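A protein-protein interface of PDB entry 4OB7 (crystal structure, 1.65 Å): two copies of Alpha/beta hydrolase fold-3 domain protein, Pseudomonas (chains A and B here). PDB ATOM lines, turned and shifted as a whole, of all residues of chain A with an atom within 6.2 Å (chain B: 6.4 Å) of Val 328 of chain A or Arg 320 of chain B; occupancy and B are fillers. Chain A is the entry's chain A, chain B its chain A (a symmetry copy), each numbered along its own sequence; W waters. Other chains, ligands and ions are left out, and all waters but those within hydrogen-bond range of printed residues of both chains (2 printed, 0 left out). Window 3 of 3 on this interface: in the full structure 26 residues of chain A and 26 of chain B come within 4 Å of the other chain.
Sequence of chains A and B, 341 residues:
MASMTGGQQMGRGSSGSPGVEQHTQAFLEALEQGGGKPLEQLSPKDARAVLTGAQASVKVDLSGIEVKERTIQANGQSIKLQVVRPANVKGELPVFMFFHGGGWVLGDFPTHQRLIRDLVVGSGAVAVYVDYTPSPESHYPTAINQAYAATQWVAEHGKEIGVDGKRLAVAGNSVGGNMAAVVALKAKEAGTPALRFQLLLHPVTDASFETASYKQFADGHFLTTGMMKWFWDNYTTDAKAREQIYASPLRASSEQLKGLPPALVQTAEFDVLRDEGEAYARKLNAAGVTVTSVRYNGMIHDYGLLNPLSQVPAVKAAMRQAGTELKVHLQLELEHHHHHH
O of Glu 325 of chain A is in hydrogen-bond range of ND1 of His 329 of chain A (2.7 Å). The backbone carbonyl oxygen (O) of Val 328 of chain A sits at hydrogen-bond distance from the side-chain amide nitrogen (NE2) of Gln 331 of chain A, at 2.9 Å. OG1 of Thr 324 of chain B is in hydrogen-bond range of O of Arg 320 of chain B (3.1 Å).
Positions printed for both chains: 323, 324 and 325. Of the 6 pairs that touch across the chains among the printed residues, none has its exchanged pair printed and touching as well.
Of the 11 printed residues of chain A, 4 touch a printed residue of chain B. Hydrophobic or aromatic side chains of chain A within 4 Å of the printed part of chain B: Val 328. Hydrophobic or aromatic side chains of chain B that line the printed part of chain A: Ala 317. Among the printed residues, 6 pairs touch across the chains. Among the printed residues, Asp or Glu carboxylates within 4 Å of a Lys or Arg side-chain nitrogen of the other chain: Glu 325 of chain A with Arg 320 of chain B (2.8 Å).
Of the printed residues of chain B, Thr 292 of chain A touches Pro 313 (3.96 Å) and Ala 317 (3.9 Å). Of the printed residues of chain B, Glu 325 of chain A touches Ala 317 (3.7 Å) and Arg 320 (2.8 Å). Printed residues of chain B within 4 Å of Val 328 of chain A: Arg 320. His 329 of chain A touches none of the printed residues of chain B. Of chain A, only Thr 324 (3.95 Å), Glu 325 (2.8 Å) and Val 328 (3.6 Å) come within 4 Å of Arg 320 of chain B. Glu 325 of chain B touches none of the printed residues of chain A. The nearest residue of chain A that does not touch Arg 320 of chain B is His 329 of chain A (4.7 Å).
Among the printed residues, merely in contact across the chains: Val 328 of chain A with Arg 320 of chain B, Glu 325 of chain A with Ala 317 of chain B, Thr 292 of chain A with Ala 317 of chain B, Thr 324 of chain A with Arg 320 of chain B and Thr 292 of chain A with Pro 313 of chain B.
Water W1 bridges the side-chain hydroxyl (OG1) of Thr 324 of chain A and the side-chain hydroxyl (OG1) of Thr 324 of chain B. Water W2 lies within hydrogen-bond range of O of Ala 317 of chain B (2.8 Å) and OE2 of Glu 325 of chain A (2.8 Å).
The side-chain carboxylate (OE1) of Glu 325 of chain A is in salt-bridge range of the guanidinium group (NH2) of Arg 320 of chain B (2.8 Å).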
ATOM      1  N   ARG A 196     -38.926   7.991 -23.103  1.00  0.00           N
ATOM      2  CA  ARG A 196     -37.808   7.130 -22.743  1.00  0.00           C
ATOM      3  C   ARG A 196     -36.606   7.298 -23.659  1.00  0.00           C
ATOM      4  O   ARG A 196     -35.473   7.026 -23.251  1.00  0.00           O
ATOM      5  CB  ARG A 196     -38.243   5.660 -22.808  1.00  0.00           C
ATOM      6  CG  ARG A 196     -39.102   5.190 -21.626  1.00  0.00           C
ATOM      7  CD  ARG A 196     -38.273   5.019 -20.362  1.00  0.00           C
ATOM      8  NE  ARG A 196     -39.003   4.275 -19.326  1.00  0.00           N
ATOM      9  CZ  ARG A 196     -39.003   2.951 -19.220  1.00  0.00           C
ATOM     10  NH1 ARG A 196     -38.337   2.216 -20.093  1.00  0.00           N
ATOM     11  NH2 ARG A 196     -39.684   2.358 -18.243  1.00  0.00           N
ATOM     12  N   THR A 292     -25.902   8.254 -28.032  1.00  0.00           N
ATOM     13  CA  THR A 292     -25.066   7.330 -28.783  1.00  0.00           C
ATOM     14  C   THR A 292     -25.155   7.816 -30.220  1.00  0.00           C
ATOM     15  O   THR A 292     -26.250   7.900 -30.781  1.00  0.00           O
ATOM     16  CB  THR A 292     -25.598   5.887 -28.662  1.00  0.00           C
ATOM     17  OG1 THR A 292     -25.587   5.501 -27.280  1.00  0.00           O
ATOM     18  CG2 THR A 292     -24.722   4.901 -29.455  1.00  0.00           C
ATOM     19  N   GLY A 323     -33.554  -1.442 -33.596  1.00  0.00           N
ATOM     20  CA  GLY A 323     -34.564  -2.200 -32.875  1.00  0.00           C
ATOM     21  C   GLY A 323     -34.123  -2.535 -31.462  1.00  0.00           C
ATOM     22  O   GLY A 323     -34.891  -2.405 -30.505  1.00  0.00           O
ATOM     23  N   THR A 324     -32.873  -2.967 -31.334  1.00  0.00           N
ATOM     24  CA  THR A 324     -32.315  -3.300 -30.026  1.00  0.00           C
ATOM     25  C   THR A 324     -32.286  -2.107 -29.078  1.00  0.00           C
ATOM     26  O   THR A 324     -32.637  -2.235 -27.907  1.00  0.00           O
ATOM     27  CB  THR A 324     -30.907  -3.891 -30.165  1.00  0.00           C
ATOM     28  OG1 THR A 324     -31.027  -5.223 -30.674  1.00  0.00           O
ATOM     29  CG2 THR A 324     -30.191  -3.933 -28.814  1.00  0.00           C
ATOM     30  N   GLU A 325     -31.886  -0.946 -29.580  1.00  0.00           N
ATOM     31  CA  GLU A 325     -31.825   0.228 -28.721  1.00  0.00           C
ATOM     32  C   GLU A 325     -33.218   0.700 -28.304  1.00  0.00           C
ATOM     33  O   GLU A 325     -33.408   1.126 -27.174  1.00  0.00           O
ATOM     34  CB  GLU A 325     -30.988   1.333 -29.368  1.00  0.00           C
ATOM     35  CG  GLU A 325     -29.536   0.881 -29.614  1.00  0.00           C
ATOM     36  CD  GLU A 325     -28.838   0.435 -28.340  1.00  0.00           C
ATOM     37  OE1 GLU A 325     -28.929   1.165 -27.327  1.00  0.00           O
ATOM     38  OE2 GLU A 325     -28.200  -0.647 -28.336  1.00  0.00           O
ATOM     39  N   LEU A 326     -34.193   0.611 -29.203  1.00  0.00           N
ATOM     40  CA  LEU A 326     -35.587   0.829 -28.804  1.00  0.00           C
ATOM     41  C   LEU A 326     -35.962  -0.104 -27.654  1.00  0.00           C
ATOM     42  O   LEU A 326     -36.470   0.335 -26.621  1.00  0.00           O
ATOM     43  CB  LEU A 326     -36.527   0.603 -29.989  1.00  0.00           C
ATOM     44  CG  LEU A 326     -36.598   1.744 -31.006  1.00  0.00           C
ATOM     45  CD1 LEU A 326     -37.311   1.275 -32.272  1.00  0.00           C
ATOM     46  CD2 LEU A 326     -37.324   2.949 -30.399  1.00  0.00           C
ATOM     47  N   LYS A 327     -35.687  -1.393 -27.826  1.00  0.00           N
ATOM     48  CA  LYS A 327     -36.057  -2.395 -26.824  1.00  0.00           C
ATOM     49  C   LYS A 327     -35.412  -2.090 -25.473  1.00  0.00           C
ATOM     50  O   LYS A 327     -36.084  -2.110 -24.424  1.00  0.00           O
ATOM     51  CB  LYS A 327     -35.637  -3.789 -27.301  1.00  0.00           C
ATOM     52  CG  LYS A 327     -36.055  -4.927 -26.383  1.00  0.00           C
ATOM     53  CD  LYS A 327     -35.618  -6.261 -26.987  1.00  0.00           C
ATOM     54  CE  LYS A 327     -36.072  -7.438 -26.141  1.00  0.00           C
ATOM     55  NZ  LYS A 327     -35.687  -8.726 -26.788  1.00  0.00           N
ATOM     56  N   VAL A 328     -34.116  -1.798 -25.496  1.00  0.00           N
ATOM     57  CA  VAL A 328     -33.366  -1.522 -24.273  1.00  0.00           C
ATOM     58  C   VAL A 328     -33.964  -0.362 -23.491  1.00  0.00           C
ATOM     59  O   VAL A 328     -34.026  -0.398 -22.255  1.00  0.00           O
ATOM     60  CB  VAL A 328     -31.881  -1.227 -24.599  1.00  0.00           C
ATOM     61  CG1 VAL A 328     -31.182  -0.548 -23.424  1.00  0.00           C
ATOM     62  CG2 VAL A 328     -31.179  -2.512 -24.971  1.00  0.00           C
ATOM     63  N   HIS A 329     -34.417   0.661 -24.212  1.00  0.00           N
ATOM     64  CA  HIS A 329     -34.889   1.874 -23.558  1.00  0.00           C
ATOM     65  C   HIS A 329     -36.362   1.843 -23.185  1.00  0.00           C
ATOM     66  O   HIS A 329     -36.832   2.744 -22.496  1.00  0.00           O
ATOM     67  CB  HIS A 329     -34.584   3.102 -24.413  1.00  0.00           C
ATOM     68  CG  HIS A 329     -33.128   3.433 -24.469  1.00  0.00           C
ATOM     69  ND1 HIS A 329     -32.264   2.837 -25.365  1.00  0.00           N
ATOM     70  CD2 HIS A 329     -32.376   4.275 -23.722  1.00  0.00           C
ATOM     71  CE1 HIS A 329     -31.045   3.309 -25.175  1.00  0.00           C
ATOM     72  NE2 HIS A 329     -31.085   4.184 -24.186  1.00  0.00           N
ATOM     73  N   LEU A 330     -37.075   0.808 -23.625  1.00  0.00           N
ATOM     74  CA  LEU A 330     -38.517   0.705 -23.381  1.00  0.00           C
ATOM     75  C   LEU A 330     -38.879  -0.381 -22.364  1.00  0.00           C
ATOM     76  O   LEU A 330     -40.054  -0.709 -22.189  1.00  0.00           O
ATOM     77  CB  LEU A 330     -39.253   0.463 -24.709  1.00  0.00           C
ATOM     78  CG  LEU A 330     -39.253   1.665 -25.658  1.00  0.00           C
ATOM     79  CD1 LEU A 330     -39.841   1.308 -27.016  1.00  0.00           C
ATOM     80  CD2 LEU A 330     -40.035   2.810 -25.045  1.00  0.00           C
ATOM     81  N   GLN A 331     -37.870  -0.947 -21.709  1.00  0.00           N
ATOM     82  CA  GLN A 331     -38.086  -1.998 -20.717  1.00  0.00           C
ATOM     83  C   GLN A 331     -38.860  -1.517 -19.508  1.00  0.00           C
ATOM     84  O   GLN A 331     -38.876  -0.330 -19.190  1.00  0.00           O
ATOM     85  CB  GLN A 331     -36.755  -2.490 -20.158  1.00  0.00           C
ATOM     86  CG  GLN A 331     -35.838  -3.208 -21.074  1.00  0.00           C
ATOM     87  CD  GLN A 331     -34.521  -3.488 -20.363  1.00  0.00           C
ATOM     88  OE1 GLN A 331     -34.461  -4.326 -19.461  1.00  0.00           O
ATOM     89  NE2 GLN A 331     -33.473  -2.751 -20.727  1.00  0.00           N
ATOM     90  N   GLY B 122     -23.495 -11.379 -24.707  1.00  0.00           N
ATOM     91  CA  GLY B 122     -24.279 -10.714 -25.731  1.00  0.00           C
ATOM     92  C   GLY B 122     -24.443 -11.503 -27.016  1.00  0.00           C
ATOM     93  O   GLY B 122     -25.309 -11.177 -27.818  1.00  0.00           O
ATOM     94  N   PRO B 313     -23.234   4.840 -21.790  1.00  0.00           N
ATOM     95  CA  PRO B 313     -24.308   4.278 -22.622  1.00  0.00           C
ATOM     96  C   PRO B 313     -23.889   3.948 -24.056  1.00  0.00           C
ATOM     97  O   PRO B 313     -24.284   2.898 -24.547  1.00  0.00           O
ATOM     98  CB  PRO B 313     -25.385   5.366 -22.580  1.00  0.00           C
ATOM     99  CG  PRO B 313     -25.181   5.997 -21.209  1.00  0.00           C
ATOM    100  CD  PRO B 313     -23.679   6.029 -21.037  1.00  0.00           C
ATOM    101  N   VAL B 315     -21.005   3.015 -25.025  1.00  0.00           N
ATOM    102  CA  VAL B 315     -20.165   1.823 -24.957  1.00  0.00           C
ATOM    103  C   VAL B 315     -21.048   0.584 -24.824  1.00  0.00           C
ATOM    104  O   VAL B 315     -20.803  -0.441 -25.472  1.00  0.00           O
ATOM    105  CB  VAL B 315     -19.163   1.908 -23.783  1.00  0.00           C
ATOM    106  CG1 VAL B 315     -18.451   0.581 -23.595  1.00  0.00           C
ATOM    107  CG2 VAL B 315     -18.156   3.021 -24.039  1.00  0.00           C
ATOM    108  N   LYS B 316     -22.088   0.679 -24.001  1.00  0.00           N
ATOM    109  CA  LYS B 316     -23.015  -0.434 -23.848  1.00  0.00           C
ATOM    110  C   LYS B 316     -23.693  -0.744 -25.178  1.00  0.00           C
ATOM    111  O   LYS B 316     -23.857  -1.906 -25.539  1.00  0.00           O
ATOM    112  CB  LYS B 316     -24.034  -0.152 -22.735  1.00  0.00           C
ATOM    113  CG  LYS B 316     -23.384  -0.041 -21.354  1.00  0.00           C
ATOM    114  CD  LYS B 316     -24.412   0.163 -20.250  1.00  0.00           C
ATOM    115  CE  LYS B 316     -25.263  -1.076 -20.063  1.00  0.00           C
ATOM    116  NZ  LYS B 316     -24.459  -2.199 -19.505  1.00  0.00           N
ATOM    117  N   ALA B 317     -24.045   0.296 -25.926  1.00  0.00           N
ATOM    118  CA  ALA B 317     -24.637   0.096 -27.247  1.00  0.00           C
ATOM    119  C   ALA B 317     -23.654  -0.577 -28.204  1.00  0.00           C
ATOM    120  O   ALA B 317     -24.026  -1.481 -28.958  1.00  0.00           O
ATOM    121  CB  ALA B 317     -25.116   1.421 -27.821  1.00  0.00           C
ATOM    122  N   ALA B 318     -22.394  -0.138 -28.177  1.00  0.00           N
ATOM    123  CA  ALA B 318     -21.372  -0.737 -29.030  1.00  0.00           C
ATOM    124  C   ALA B 318     -21.182  -2.209 -28.695  1.00  0.00           C
ATOM    125  O   ALA B 318     -21.005  -3.038 -29.586  1.00  0.00           O
ATOM    126  CB  ALA B 318     -20.040   0.014 -28.895  1.00  0.00           C
ATOM    127  N   MET B 319     -21.218  -2.530 -27.405  1.00  0.00           N
ATOM    128  CA  MET B 319     -21.063  -3.914 -26.960  1.00  0.00           C
ATOM    129  C   MET B 319     -22.274  -4.762 -27.325  1.00  0.00           C
ATOM    130  O   MET B 319     -22.126  -5.924 -27.708  1.00  0.00           O
ATOM    131  CB  MET B 319     -20.802  -3.979 -25.449  1.00  0.00           C
ATOM    132  CG  MET B 319     -19.508  -3.317 -25.005  1.00  0.00           C
ATOM    133  SD  MET B 319     -18.042  -4.148 -25.641  1.00  0.00           S
ATOM    134  CE  MET B 319     -17.636  -3.118 -27.019  1.00  0.00           C
ATOM    135  N   ARG B 320     -23.470  -4.194 -27.209  1.00  0.00           N
ATOM    136  CA  ARG B 320     -24.665  -4.900 -27.661  1.00  0.00           C
ATOM    137  C   ARG B 320     -24.563  -5.234 -29.144  1.00  0.00           C
ATOM    138  O   ARG B 320     -24.878  -6.353 -29.554  1.00  0.00           O
ATOM    139  CB  ARG B 320     -25.927  -4.074 -27.395  1.00  0.00           C
ATOM    140  CG  ARG B 320     -26.371  -4.099 -25.946  1.00  0.00           C
ATOM    141  CD  ARG B 320     -27.725  -3.442 -25.763  1.00  0.00           C
ATOM    142  NE  ARG B 320     -27.722  -1.979 -25.881  1.00  0.00           N
ATOM    143  CZ  ARG B 320     -27.532  -1.143 -24.863  1.00  0.00           C
ATOM    144  NH1 ARG B 320     -27.276  -1.613 -23.642  1.00  0.00           N
ATOM    145  NH2 ARG B 320     -27.582   0.166 -25.067  1.00  0.00           N
ATOM    146  N   GLN B 321     -24.113  -4.272 -29.946  1.00  0.00           N
ATOM    147  CA  GLN B 321     -23.964  -4.514 -31.380  1.00  0.00           C
ATOM    148  C   GLN B 321     -22.935  -5.595 -31.677  1.00  0.00           C
ATOM    149  O   GLN B 321     -23.179  -6.492 -32.486  1.00  0.00           O
ATOM    150  CB  GLN B 321     -23.572  -3.237 -32.120  1.00  0.00           C
ATOM    151  CG  GLN B 321     -23.205  -3.502 -33.571  1.00  0.00           C
ATOM    152  CD  GLN B 321     -23.101  -2.238 -34.368  1.00  0.00           C
ATOM    153  OE1 GLN B 321     -22.168  -1.446 -34.185  1.00  0.00           O
ATOM    154  NE2 GLN B 321     -24.070  -2.021 -35.258  1.00  0.00           N
ATOM    155  N   ALA B 322     -21.781  -5.507 -31.025  1.00  0.00           N
ATOM    156  CA  ALA B 322     -20.721  -6.480 -31.275  1.00  0.00           C
ATOM    157  C   ALA B 322     -21.178  -7.908 -30.954  1.00  0.00           C
ATOM    158  O   ALA B 322     -20.910  -8.831 -31.728  1.00  0.00           O
ATOM    159  CB  ALA B 322     -19.450  -6.109 -30.507  1.00  0.00           C
ATOM    160  N   GLY B 323     -21.878  -8.085 -29.833  1.00  0.00           N
ATOM    161  CA  GLY B 323     -22.395  -9.392 -29.461  1.00  0.00           C
ATOM    162  C   GLY B 323     -23.449  -9.885 -30.435  1.00  0.00           C
ATOM    163  O   GLY B 323     -23.445 -11.049 -30.846  1.00  0.00           O
ATOM    164  N   THR B 324     -24.355  -8.988 -30.810  1.00  0.00           N
ATOM    165  CA  THR B 324     -25.409  -9.326 -31.763  1.00  0.00           C
ATOM    166  C   THR B 324     -24.860  -9.738 -33.124  1.00  0.00           C
ATOM    167  O   THR B 324     -25.324 -10.713 -33.712  1.00  0.00           O
ATOM    168  CB  THR B 324     -26.393  -8.162 -31.928  1.00  0.00           C
ATOM    169  OG1 THR B 324     -27.205  -8.091 -30.752  1.00  0.00           O
ATOM    170  CG2 THR B 324     -27.292  -8.368 -33.147  1.00  0.00           C
ATOM    171  N   GLU B 325     -23.866  -9.014 -33.620  1.00  0.00           N
ATOM    172  CA  GLU B 325     -23.308  -9.350 -34.921  1.00  0.00           C
ATOM    173  C   GLU B 325     -22.545 -10.674 -34.888  1.00  0.00           C
ATOM    174  O   GLU B 325     -22.608 -11.442 -35.837  1.00  0.00           O
ATOM    175  CB  GLU B 325     -22.472  -8.193 -35.472  1.00  0.00           C
ATOM    176  CG  GLU B 325     -23.315  -6.917 -35.661  1.00  0.00           C
ATOM    177  CD  GLU B 325     -24.503  -7.133 -36.585  1.00  0.00           C
ATOM    178  OE1 GLU B 325     -24.309  -7.724 -37.671  1.00  0.00           O
ATOM    179  OE2 GLU B 325     -25.636  -6.721 -36.235  1.00  0.00           O
HETATM  180  O   HOH W   1     -28.583  -5.936 -31.094  1.00  0.00           O
HETATM  181  O   HOH W   2     -26.430  -1.490 -30.342  1.00  0.00           O
